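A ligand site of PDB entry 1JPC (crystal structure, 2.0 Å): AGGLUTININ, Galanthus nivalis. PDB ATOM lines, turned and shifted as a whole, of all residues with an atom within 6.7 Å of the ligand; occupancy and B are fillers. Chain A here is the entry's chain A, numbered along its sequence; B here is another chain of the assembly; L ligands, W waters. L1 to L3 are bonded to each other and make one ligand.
The side-chain carboxylate (OD2) of Asp 37 of chain B is in hydrogen-bond range of an oxygen (O1) of LIG L1 (2.7 Å). An oxygen (O4) of LG2 L2 is in hydrogen-bond range of the side-chain hydroxyl of Tyr 34 (2.8 Å). O2 of LG2 L2 is in hydrogen-bond range of OD2 of Asp 28 (2.8 Å). ND2 of Asn 30 sits at hydrogen-bond distance from O5 of LG2 L2 (2.8 Å). The side-chain amino group of Lys 38 of chain B sits at hydrogen-bond distance from an oxygen (O2) of LIG L1, 2.8 Å away. The side-chain amide oxygen (OD1) of Asn 44 lies within hydrogen-bond range of an oxygen (O3) of LG3 L3 (3.1 Å). An oxygen (O3) of LG2 L2 lies close to the side-chain amide oxygen of Gln 26 (3.2 Å). O of Pro 39 sits at hydrogen-bond distance from O5 of LG3 L3.
The side-chain amino group (NZ) of Lys 38 of chain B is in salt-bridge range of the side-chain carboxylate (OD1) of Asp 37 of chain B (2.7 Å). The side-chain hydroxyl (OH) of Tyr 34 is in hydrogen-bond range of the side-chain amide nitrogen (NE2) of Gln 26 (2.7 Å). OD1 of Asp 28 sits at hydrogen-bond distance from N of Asn 30, 3.1 Å away. OD1 of Asp 28 sits close to OE1 of Gln 26, at 3.3 Å. The backbone NH (N) of Gly 47 lies within hydrogen-bond range of the backbone carbonyl oxygen (O) of Asp 28 (2.9 Å). The side-chain amide oxygen (OD1) of Asn 30 lies within hydrogen-bond range of the backbone NH (N) of Asn 44 (2.9 Å). OD1 of Asn 30 is in hydrogen-bond range of N of Thr 45 (3.1 Å). N of Leu 33 sits at hydrogen-bond distance from O of Trp 41 (2.8 Å).
Merely in contact with the ligand: Trp 41 (3.8 Å), Ile 40 (3.9 Å) and Ala 42 (3.98 Å). 11 residues have an atom within 4 Å of the ligand: Gln 26, Asp 28, Asn 30, Tyr 34, Pro 39, Ile 40, Trp 41, Ala 42, Asn 44, Asp 37 of chain B and Lys 38 of chain B. Along chain A the residues within 4 Å of the ligand span positions 26 to 44.
Water W4 lies within hydrogen-bond range of O3 of LIG L1, N of Glu 27 and N of Asp 28. Water W3 lies within hydrogen-bond range of OD1 of Asn 44 (2.6 Å), O6 of LG2 L2 (2.8 Å) and ND2 of Asn 30 (3.1 Å). Water W2 lies within hydrogen-bond range of NE2 of Gln 26, OD1 of Asp 37 of chain B, O2 of LIG L1 and NZ of Lys 38 of chain B.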
ATOM      1  N   GLN A  26      18.381 -19.217 -14.757  1.00  0.00           N
ATOM      2  CA  GLN A  26      19.488 -18.886 -15.650  1.00  0.00           C
ATOM      3  C   GLN A  26      19.155 -17.974 -16.833  1.00  0.00           C
ATOM      4  O   GLN A  26      18.001 -17.832 -17.233  1.00  0.00           O
ATOM      5  CB  GLN A  26      20.166 -20.158 -16.140  1.00  0.00           C
ATOM      6  CG  GLN A  26      20.762 -20.970 -15.017  1.00  0.00           C
ATOM      7  CD  GLN A  26      21.404 -22.229 -15.503  1.00  0.00           C
ATOM      8  OE1 GLN A  26      21.207 -22.656 -16.632  1.00  0.00           O
ATOM      9  NE2 GLN A  26      22.207 -22.845 -14.654  1.00  0.00           N
ATOM     10  N   GLU A  27      20.193 -17.345 -17.385  1.00  0.00           N
ATOM     11  CA  GLU A  27      20.000 -16.440 -18.509  1.00  0.00           C
ATOM     12  C   GLU A  27      19.598 -17.159 -19.778  1.00  0.00           C
ATOM     13  O   GLU A  27      19.021 -16.552 -20.679  1.00  0.00           O
ATOM     14  CB  GLU A  27      21.209 -15.537 -18.745  1.00  0.00           C
ATOM     15  CG  GLU A  27      20.835 -14.327 -19.610  1.00  0.00           C
ATOM     16  CD  GLU A  27      21.894 -13.237 -19.668  1.00  0.00           C
ATOM     17  OE1 GLU A  27      22.612 -13.034 -18.674  1.00  0.00           O
ATOM     18  OE2 GLU A  27      21.988 -12.579 -20.730  1.00  0.00           O
ATOM     19  N   ASP A  28      19.864 -18.460 -19.850  1.00  0.00           N
ATOM     20  CA  ASP A  28      19.471 -19.233 -21.016  1.00  0.00           C
ATOM     21  C   ASP A  28      18.051 -19.787 -20.818  1.00  0.00           C
ATOM     22  O   ASP A  28      17.649 -20.735 -21.477  1.00  0.00           O
ATOM     23  CB  ASP A  28      20.472 -20.363 -21.288  1.00  0.00           C
ATOM     24  CG  ASP A  28      20.419 -21.468 -20.249  1.00  0.00           C
ATOM     25  OD1 ASP A  28      19.735 -21.309 -19.211  1.00  0.00           O
ATOM     26  OD2 ASP A  28      21.064 -22.509 -20.467  1.00  0.00           O
ATOM     27  N   CYS A  29      17.318 -19.194 -19.873  1.00  0.00           N
ATOM     28  CA  CYS A  29      15.940 -19.573 -19.560  1.00  0.00           C
ATOM     29  C   CYS A  29      15.711 -20.956 -18.968  1.00  0.00           C
ATOM     30  O   CYS A  29      14.567 -21.424 -18.900  1.00  0.00           O
ATOM     31  CB  CYS A  29      14.994 -19.372 -20.760  1.00  0.00           C
ATOM     32  SG  CYS A  29      14.652 -17.619 -21.123  1.00  0.00           S
ATOM     33  N   ASN A  30      16.773 -21.621 -18.530  1.00  0.00           N
ATOM     34  CA  ASN A  30      16.624 -22.926 -17.900  1.00  0.00           C
ATOM     35  C   ASN A  30      16.556 -22.662 -16.382  1.00  0.00           C
ATOM     36  O   ASN A  30      17.313 -21.833 -15.857  1.00  0.00           O
ATOM     37  CB  ASN A  30      17.823 -23.812 -18.237  1.00  0.00           C
ATOM     38  CG  ASN A  30      17.507 -25.290 -18.106  1.00  0.00           C
ATOM     39  OD1 ASN A  30      16.361 -25.689 -17.920  1.00  0.00           O
ATOM     40  ND2 ASN A  30      18.544 -26.124 -18.198  1.00  0.00           N
ATOM     41  N   LEU A  31      15.565 -23.242 -15.706  1.00  0.00           N
ATOM     42  CA  LEU A  31      15.428 -23.098 -14.258  1.00  0.00           C
ATOM     43  C   LEU A  31      16.052 -24.375 -13.704  1.00  0.00           C
ATOM     44  O   LEU A  31      15.533 -25.466 -13.926  1.00  0.00           O
ATOM     45  CB  LEU A  31      13.958 -22.996 -13.877  1.00  0.00           C
ATOM     46  CG  LEU A  31      13.615 -22.933 -12.382  1.00  0.00           C
ATOM     47  CD1 LEU A  31      14.327 -21.772 -11.703  1.00  0.00           C
ATOM     48  CD2 LEU A  31      12.120 -22.765 -12.247  1.00  0.00           C
ATOM     49  N   VAL A  32      17.182 -24.236 -13.006  1.00  0.00           N
ATOM     50  CA  VAL A  32      17.900 -25.406 -12.507  1.00  0.00           C
ATOM     51  C   VAL A  32      18.188 -25.458 -11.007  1.00  0.00           C
ATOM     52  O   VAL A  32      18.514 -24.453 -10.384  1.00  0.00           O
ATOM     53  CB  VAL A  32      19.279 -25.530 -13.223  1.00  0.00           C
ATOM     54  CG1 VAL A  32      19.891 -26.913 -13.011  1.00  0.00           C
ATOM     55  CG2 VAL A  32      19.140 -25.207 -14.713  1.00  0.00           C
ATOM     56  N   LEU A  33      18.054 -26.655 -10.452  1.00  0.00           N
ATOM     57  CA  LEU A  33      18.355 -26.902  -9.047  1.00  0.00           C
ATOM     58  C   LEU A  33      19.730 -27.574  -9.046  1.00  0.00           C
ATOM     59  O   LEU A  33      19.914 -28.603  -9.687  1.00  0.00           O
ATOM     60  CB  LEU A  33      17.342 -27.851  -8.413  1.00  0.00           C
ATOM     61  CG  LEU A  33      17.712 -28.290  -6.988  1.00  0.00           C
ATOM     62  CD1 LEU A  33      17.837 -27.088  -6.044  1.00  0.00           C
ATOM     63  CD2 LEU A  33      16.670 -29.252  -6.478  1.00  0.00           C
ATOM     64  N   TYR A  34      20.700 -26.949  -8.392  1.00  0.00           N
ATOM     65  CA  TYR A  34      22.051 -27.488  -8.327  1.00  0.00           C
ATOM     66  C   TYR A  34      22.395 -27.903  -6.925  1.00  0.00           C
ATOM     67  O   TYR A  34      21.961 -27.264  -5.960  1.00  0.00           O
ATOM     68  CB  TYR A  34      23.068 -26.399  -8.699  1.00  0.00           C
ATOM     69  CG  TYR A  34      23.152 -26.086 -10.158  1.00  0.00           C
ATOM     70  CD1 TYR A  34      23.898 -26.888 -11.012  1.00  0.00           C
ATOM     71  CD2 TYR A  34      22.471 -24.987 -10.689  1.00  0.00           C
ATOM     72  CE1 TYR A  34      23.972 -26.616 -12.368  1.00  0.00           C
ATOM     73  CE2 TYR A  34      22.535 -24.699 -12.058  1.00  0.00           C
ATOM     74  CZ  TYR A  34      23.290 -25.525 -12.884  1.00  0.00           C
ATOM     75  OH  TYR A  34      23.361 -25.249 -14.232  1.00  0.00           O
ATOM     76  N   ASP A  37      27.873 -28.324  -7.850  1.00  0.00           N
ATOM     77  CA  ASP A  37      27.976 -28.157  -9.295  1.00  0.00           C
ATOM     78  C   ASP A  37      27.139 -29.153 -10.109  1.00  0.00           C
ATOM     79  O   ASP A  37      27.096 -29.051 -11.326  1.00  0.00           O
ATOM     80  CB  ASP A  37      29.444 -28.201  -9.745  1.00  0.00           C
ATOM     81  CG  ASP A  37      30.119 -29.539  -9.436  1.00  0.00           C
ATOM     82  OD1 ASP A  37      29.870 -30.138  -8.369  1.00  0.00           O
ATOM     83  OD2 ASP A  37      30.932 -30.007 -10.261  1.00  0.00           O
ATOM     84  N   LYS A  38      26.438 -30.078  -9.450  1.00  0.00           N
ATOM     85  CA  LYS A  38      25.636 -31.071 -10.156  1.00  0.00           C
ATOM     86  C   LYS A  38      24.173 -30.637 -10.353  1.00  0.00           C
ATOM     87  O   LYS A  38      23.508 -30.260  -9.386  1.00  0.00           O
ATOM     88  CB  LYS A  38      25.619 -32.414  -9.420  1.00  0.00           C
ATOM     89  CG  LYS A  38      26.923 -32.843  -8.762  1.00  0.00           C
ATOM     90  CD  LYS A  38      28.078 -33.080  -9.744  1.00  0.00           C
ATOM     91  CE  LYS A  38      29.295 -33.652  -9.009  1.00  0.00           C
ATOM     92  NZ  LYS A  38      29.752 -32.803  -7.859  1.00  0.00           N
ATOM     93  N   PRO A  39      23.662 -30.688 -11.598  1.00  0.00           N
ATOM     94  CA  PRO A  39      22.272 -30.305 -11.846  1.00  0.00           C
ATOM     95  C   PRO A  39      21.422 -31.468 -11.311  1.00  0.00           C
ATOM     96  O   PRO A  39      21.642 -32.615 -11.685  1.00  0.00           O
ATOM     97  CB  PRO A  39      22.181 -30.261 -13.373  1.00  0.00           C
ATOM     98  CG  PRO A  39      23.574 -30.103 -13.826  1.00  0.00           C
ATOM     99  CD  PRO A  39      24.345 -30.968 -12.870  1.00  0.00           C
ATOM    100  N   ILE A  40      20.517 -31.172 -10.383  1.00  0.00           N
ATOM    101  CA  ILE A  40      19.653 -32.186  -9.788  1.00  0.00           C
ATOM    102  C   ILE A  40      18.289 -32.218 -10.465  1.00  0.00           C
ATOM    103  O   ILE A  40      17.672 -33.263 -10.582  1.00  0.00           O
ATOM    104  CB  ILE A  40      19.485 -31.924  -8.259  1.00  0.00           C
ATOM    105  CG1 ILE A  40      20.820 -32.115  -7.560  1.00  0.00           C
ATOM    106  CG2 ILE A  40      18.492 -32.878  -7.639  1.00  0.00           C
ATOM    107  CD1 ILE A  40      21.500 -33.407  -7.931  1.00  0.00           C
ATOM    108  N   TRP A  41      17.847 -31.064 -10.956  1.00  0.00           N
ATOM    109  CA  TRP A  41      16.545 -30.946 -11.605  1.00  0.00           C
ATOM    110  C   TRP A  41      16.574 -29.709 -12.484  1.00  0.00           C
ATOM    111  O   TRP A  41      17.273 -28.748 -12.183  1.00  0.00           O
ATOM    112  CB  TRP A  41      15.477 -30.756 -10.517  1.00  0.00           C
ATOM    113  CG  TRP A  41      14.065 -30.659 -11.017  1.00  0.00           C
ATOM    114  CD1 TRP A  41      13.195 -31.692 -11.239  1.00  0.00           C
ATOM    115  CD2 TRP A  41      13.359 -29.460 -11.372  1.00  0.00           C
ATOM    116  NE1 TRP A  41      12.004 -31.205 -11.704  1.00  0.00           N
ATOM    117  CE2 TRP A  41      12.075 -29.845 -11.796  1.00  0.00           C
ATOM    118  CE3 TRP A  41      13.693 -28.096 -11.364  1.00  0.00           C
ATOM    119  CZ2 TRP A  41      11.110 -28.918 -12.214  1.00  0.00           C
ATOM    120  CZ3 TRP A  41      12.739 -27.178 -11.786  1.00  0.00           C
ATOM    121  CH2 TRP A  41      11.462 -27.591 -12.204  1.00  0.00           C
ATOM    122  N   ALA A  42      15.816 -29.735 -13.575  1.00  0.00           N
ATOM    123  CA  ALA A  42      15.749 -28.588 -14.480  1.00  0.00           C
ATOM    124  C   ALA A  42      14.442 -28.645 -15.241  1.00  0.00           C
ATOM    125  O   ALA A  42      13.793 -29.687 -15.289  1.00  0.00           O
ATOM    126  CB  ALA A  42      16.936 -28.592 -15.441  1.00  0.00           C
ATOM    127  N   THR A  43      14.021 -27.488 -15.762  1.00  0.00           N
ATOM    128  CA  THR A  43      12.804 -27.392 -16.557  1.00  0.00           C
ATOM    129  C   THR A  43      13.134 -27.816 -17.985  1.00  0.00           C
ATOM    130  O   THR A  43      12.250 -28.056 -18.798  1.00  0.00           O
ATOM    131  CB  THR A  43      12.229 -25.954 -16.545  1.00  0.00           C
ATOM    132  OG1 THR A  43      13.267 -25.024 -16.897  1.00  0.00           O
ATOM    133  CG2 THR A  43      11.688 -25.586 -15.180  1.00  0.00           C
ATOM    134  N   ASN A  44      14.439 -27.880 -18.284  1.00  0.00           N
ATOM    135  CA  ASN A  44      14.955 -28.279 -19.595  1.00  0.00           C
ATOM    136  C   ASN A  44      14.438 -27.352 -20.688  1.00  0.00           C
ATOM    137  O   ASN A  44      14.022 -27.799 -21.760  1.00  0.00           O
ATOM    138  CB  ASN A  44      14.590 -29.746 -19.894  1.00  0.00           C
ATOM    139  CG  ASN A  44      15.125 -30.724 -18.850  1.00  0.00           C
ATOM    140  OD1 ASN A  44      16.309 -30.700 -18.502  1.00  0.00           O
ATOM    141  ND2 ASN A  44      14.254 -31.569 -18.347  1.00  0.00           N
ATOM    142  N   THR A  45      14.478 -26.048 -20.404  1.00  0.00           N
ATOM    143  CA  THR A  45      14.024 -25.040 -21.349  1.00  0.00           C
ATOM    144  C   THR A  45      15.159 -24.076 -21.741  1.00  0.00           C
ATOM    145  O   THR A  45      14.920 -22.931 -22.150  1.00  0.00           O
ATOM    146  CB  THR A  45      12.831 -24.232 -20.766  1.00  0.00           C
ATOM    147  OG1 THR A  45      13.197 -23.664 -19.503  1.00  0.00           O
ATOM    148  CG2 THR A  45      11.591 -25.116 -20.588  1.00  0.00           C
ATOM    149  N   GLY A  46      16.402 -24.551 -21.621  1.00  0.00           N
ATOM    150  CA  GLY A  46      17.549 -23.725 -21.983  1.00  0.00           C
ATOM    151  C   GLY A  46      17.619 -23.535 -23.478  1.00  0.00           C
ATOM    152  O   GLY A  46      17.458 -24.490 -24.231  1.00  0.00           O
ATOM    153  N   GLY A  47      17.817 -22.290 -23.914  1.00  0.00           N
ATOM    154  CA  GLY A  47      17.887 -22.008 -25.337  1.00  0.00           C
ATOM    155  C   GLY A  47      16.576 -21.578 -25.962  1.00  0.00           C
ATOM    156  O   GLY A  47      16.569 -20.976 -27.034  1.00  0.00           O
ATOM    157  N   VAL B  36      28.059 -21.077  -8.143  1.00  0.00           N
ATOM    158  CA  VAL B  36      26.990 -21.906  -8.692  1.00  0.00           C
ATOM    159  C   VAL B  36      27.697 -23.174  -9.185  1.00  0.00           C
ATOM    160  O   VAL B  36      28.312 -23.883  -8.383  1.00  0.00           O
ATOM    161  CB  VAL B  36      26.136 -21.213  -9.817  1.00  0.00           C
ATOM    162  CG1 VAL B  36      24.962 -22.105 -10.218  1.00  0.00           C
ATOM    163  CG2 VAL B  36      25.592 -19.869  -9.313  1.00  0.00           C
ATOM    164  N   ASP B  37      27.716 -23.434 -10.486  1.00  0.00           N
ATOM    165  CA  ASP B  37      28.369 -24.633 -11.000  1.00  0.00           C
ATOM    166  C   ASP B  37      29.755 -24.386 -11.610  1.00  0.00           C
ATOM    167  O   ASP B  37      30.418 -25.336 -12.000  1.00  0.00           O
ATOM    168  CB  ASP B  37      27.463 -25.357 -12.007  1.00  0.00           C
ATOM    169  CG  ASP B  37      27.143 -24.503 -13.237  1.00  0.00           C
ATOM    170  OD1 ASP B  37      26.941 -23.283 -13.110  1.00  0.00           O
ATOM    171  OD2 ASP B  37      27.080 -25.059 -14.354  1.00  0.00           O
ATOM    172  N   LYS B  38      30.217 -23.136 -11.648  1.00  0.00           N
ATOM    173  CA  LYS B  38      31.524 -22.826 -12.227  1.00  0.00           C
ATOM    174  C   LYS B  38      32.656 -22.815 -11.198  1.00  0.00           C
ATOM    175  O   LYS B  38      32.553 -22.142 -10.171  1.00  0.00           O
ATOM    176  CB  LYS B  38      31.509 -21.460 -12.916  1.00  0.00           C
ATOM    177  CG  LYS B  38      30.244 -21.084 -13.674  1.00  0.00           C
ATOM    178  CD  LYS B  38      29.934 -21.986 -14.871  1.00  0.00           C
ATOM    179  CE  LYS B  38      28.737 -21.440 -15.656  1.00  0.00           C
ATOM    180  NZ  LYS B  38      27.510 -21.240 -14.814  1.00  0.00           N
HETATM  181  C1  LIG L   1      24.785 -24.622 -17.620  1.00  0.00           C
HETATM  182  C2  LIG L   1      25.131 -23.436 -16.725  1.00  0.00           C
HETATM  183  C3  LIG L   1      24.745 -22.101 -17.375  1.00  0.00           C
HETATM  184  C4  LIG L   1      25.256 -22.017 -18.810  1.00  0.00           C
HETATM  185  C5  LIG L   1      24.808 -23.250 -19.587  1.00  0.00           C
HETATM  186  C6  LIG L   1      25.323 -23.281 -21.021  1.00  0.00           C
HETATM  187  O1  LIG L   1      26.529 -23.434 -16.461  1.00  0.00           O
HETATM  188  O2  LIG L   1      25.316 -21.033 -16.618  1.00  0.00           O
HETATM  189  O3  LIG L   1      24.771 -20.842 -19.437  1.00  0.00           O
HETATM  190  O4  LIG L   1      25.294 -24.444 -18.938  1.00  0.00           O
HETATM  191  O5  LIG L   1      26.724 -23.493 -21.049  1.00  0.00           O
HETATM  192  C1  LG2 L   2      21.447 -27.100 -19.931  1.00  0.00           C
HETATM  193  C2  LG2 L   2      22.052 -25.792 -19.408  1.00  0.00           C
HETATM  194  C3  LG2 L   2      22.952 -26.063 -18.213  1.00  0.00           C
HETATM  195  C4  LG2 L   2      22.215 -26.871 -17.152  1.00  0.00           C
HETATM  196  C5  LG2 L   2      21.598 -28.129 -17.755  1.00  0.00           C
HETATM  197  C6  LG2 L   2      20.731 -28.876 -16.765  1.00  0.00           C
HETATM  198  O1  LG2 L   2      22.440 -27.943 -20.418  1.00  0.00           O
HETATM  199  O2  LG2 L   2      21.000 -24.923 -19.029  1.00  0.00           O
HETATM  200  O3  LG2 L   2      23.396 -24.816 -17.636  1.00  0.00           O
HETATM  201  O4  LG2 L   2      23.131 -27.245 -16.124  1.00  0.00           O
HETATM  202  O5  LG2 L   2      20.750 -27.787 -18.872  1.00  0.00           O
HETATM  203  O6  LG2 L   2      20.148 -30.034 -17.419  1.00  0.00           O
HETATM  204  C1  LG3 L   3      20.811 -31.220 -17.087  1.00  0.00           C
HETATM  205  C2  LG3 L   3      20.563 -32.263 -18.175  1.00  0.00           C
HETATM  206  C3  LG3 L   3      19.088 -32.652 -18.216  1.00  0.00           C
HETATM  207  C4  LG3 L   3      18.579 -33.036 -16.825  1.00  0.00           C
HETATM  208  C5  LG3 L   3      18.970 -32.001 -15.763  1.00  0.00           C
HETATM  209  C6  LG3 L   3      18.713 -32.505 -14.354  1.00  0.00           C
HETATM  210  O1  LG3 L   3      21.365 -33.405 -17.920  1.00  0.00           O
HETATM  211  O2  LG3 L   3      18.916 -33.753 -19.088  1.00  0.00           O
HETATM  212  O3  LG3 L   3      17.166 -33.157 -16.865  1.00  0.00           O
HETATM  213  O4  LG3 L   3      20.386 -31.724 -15.839  1.00  0.00           O
HETATM  214  O5  LG3 L   3      19.513 -33.638 -14.069  1.00  0.00           O
HETATM  215  O   HOH W   1      24.285 -30.726 -20.904  1.00  0.00           O
HETATM  216  O   HOH W   2      24.580 -21.647 -13.784  1.00  0.00           O
HETATM  217  O   HOH W   3      18.207 -29.042 -19.216  1.00  0.00           O
HETATM  218  O   HOH W   4      22.855 -19.051 -18.445  1.00  0.00           O
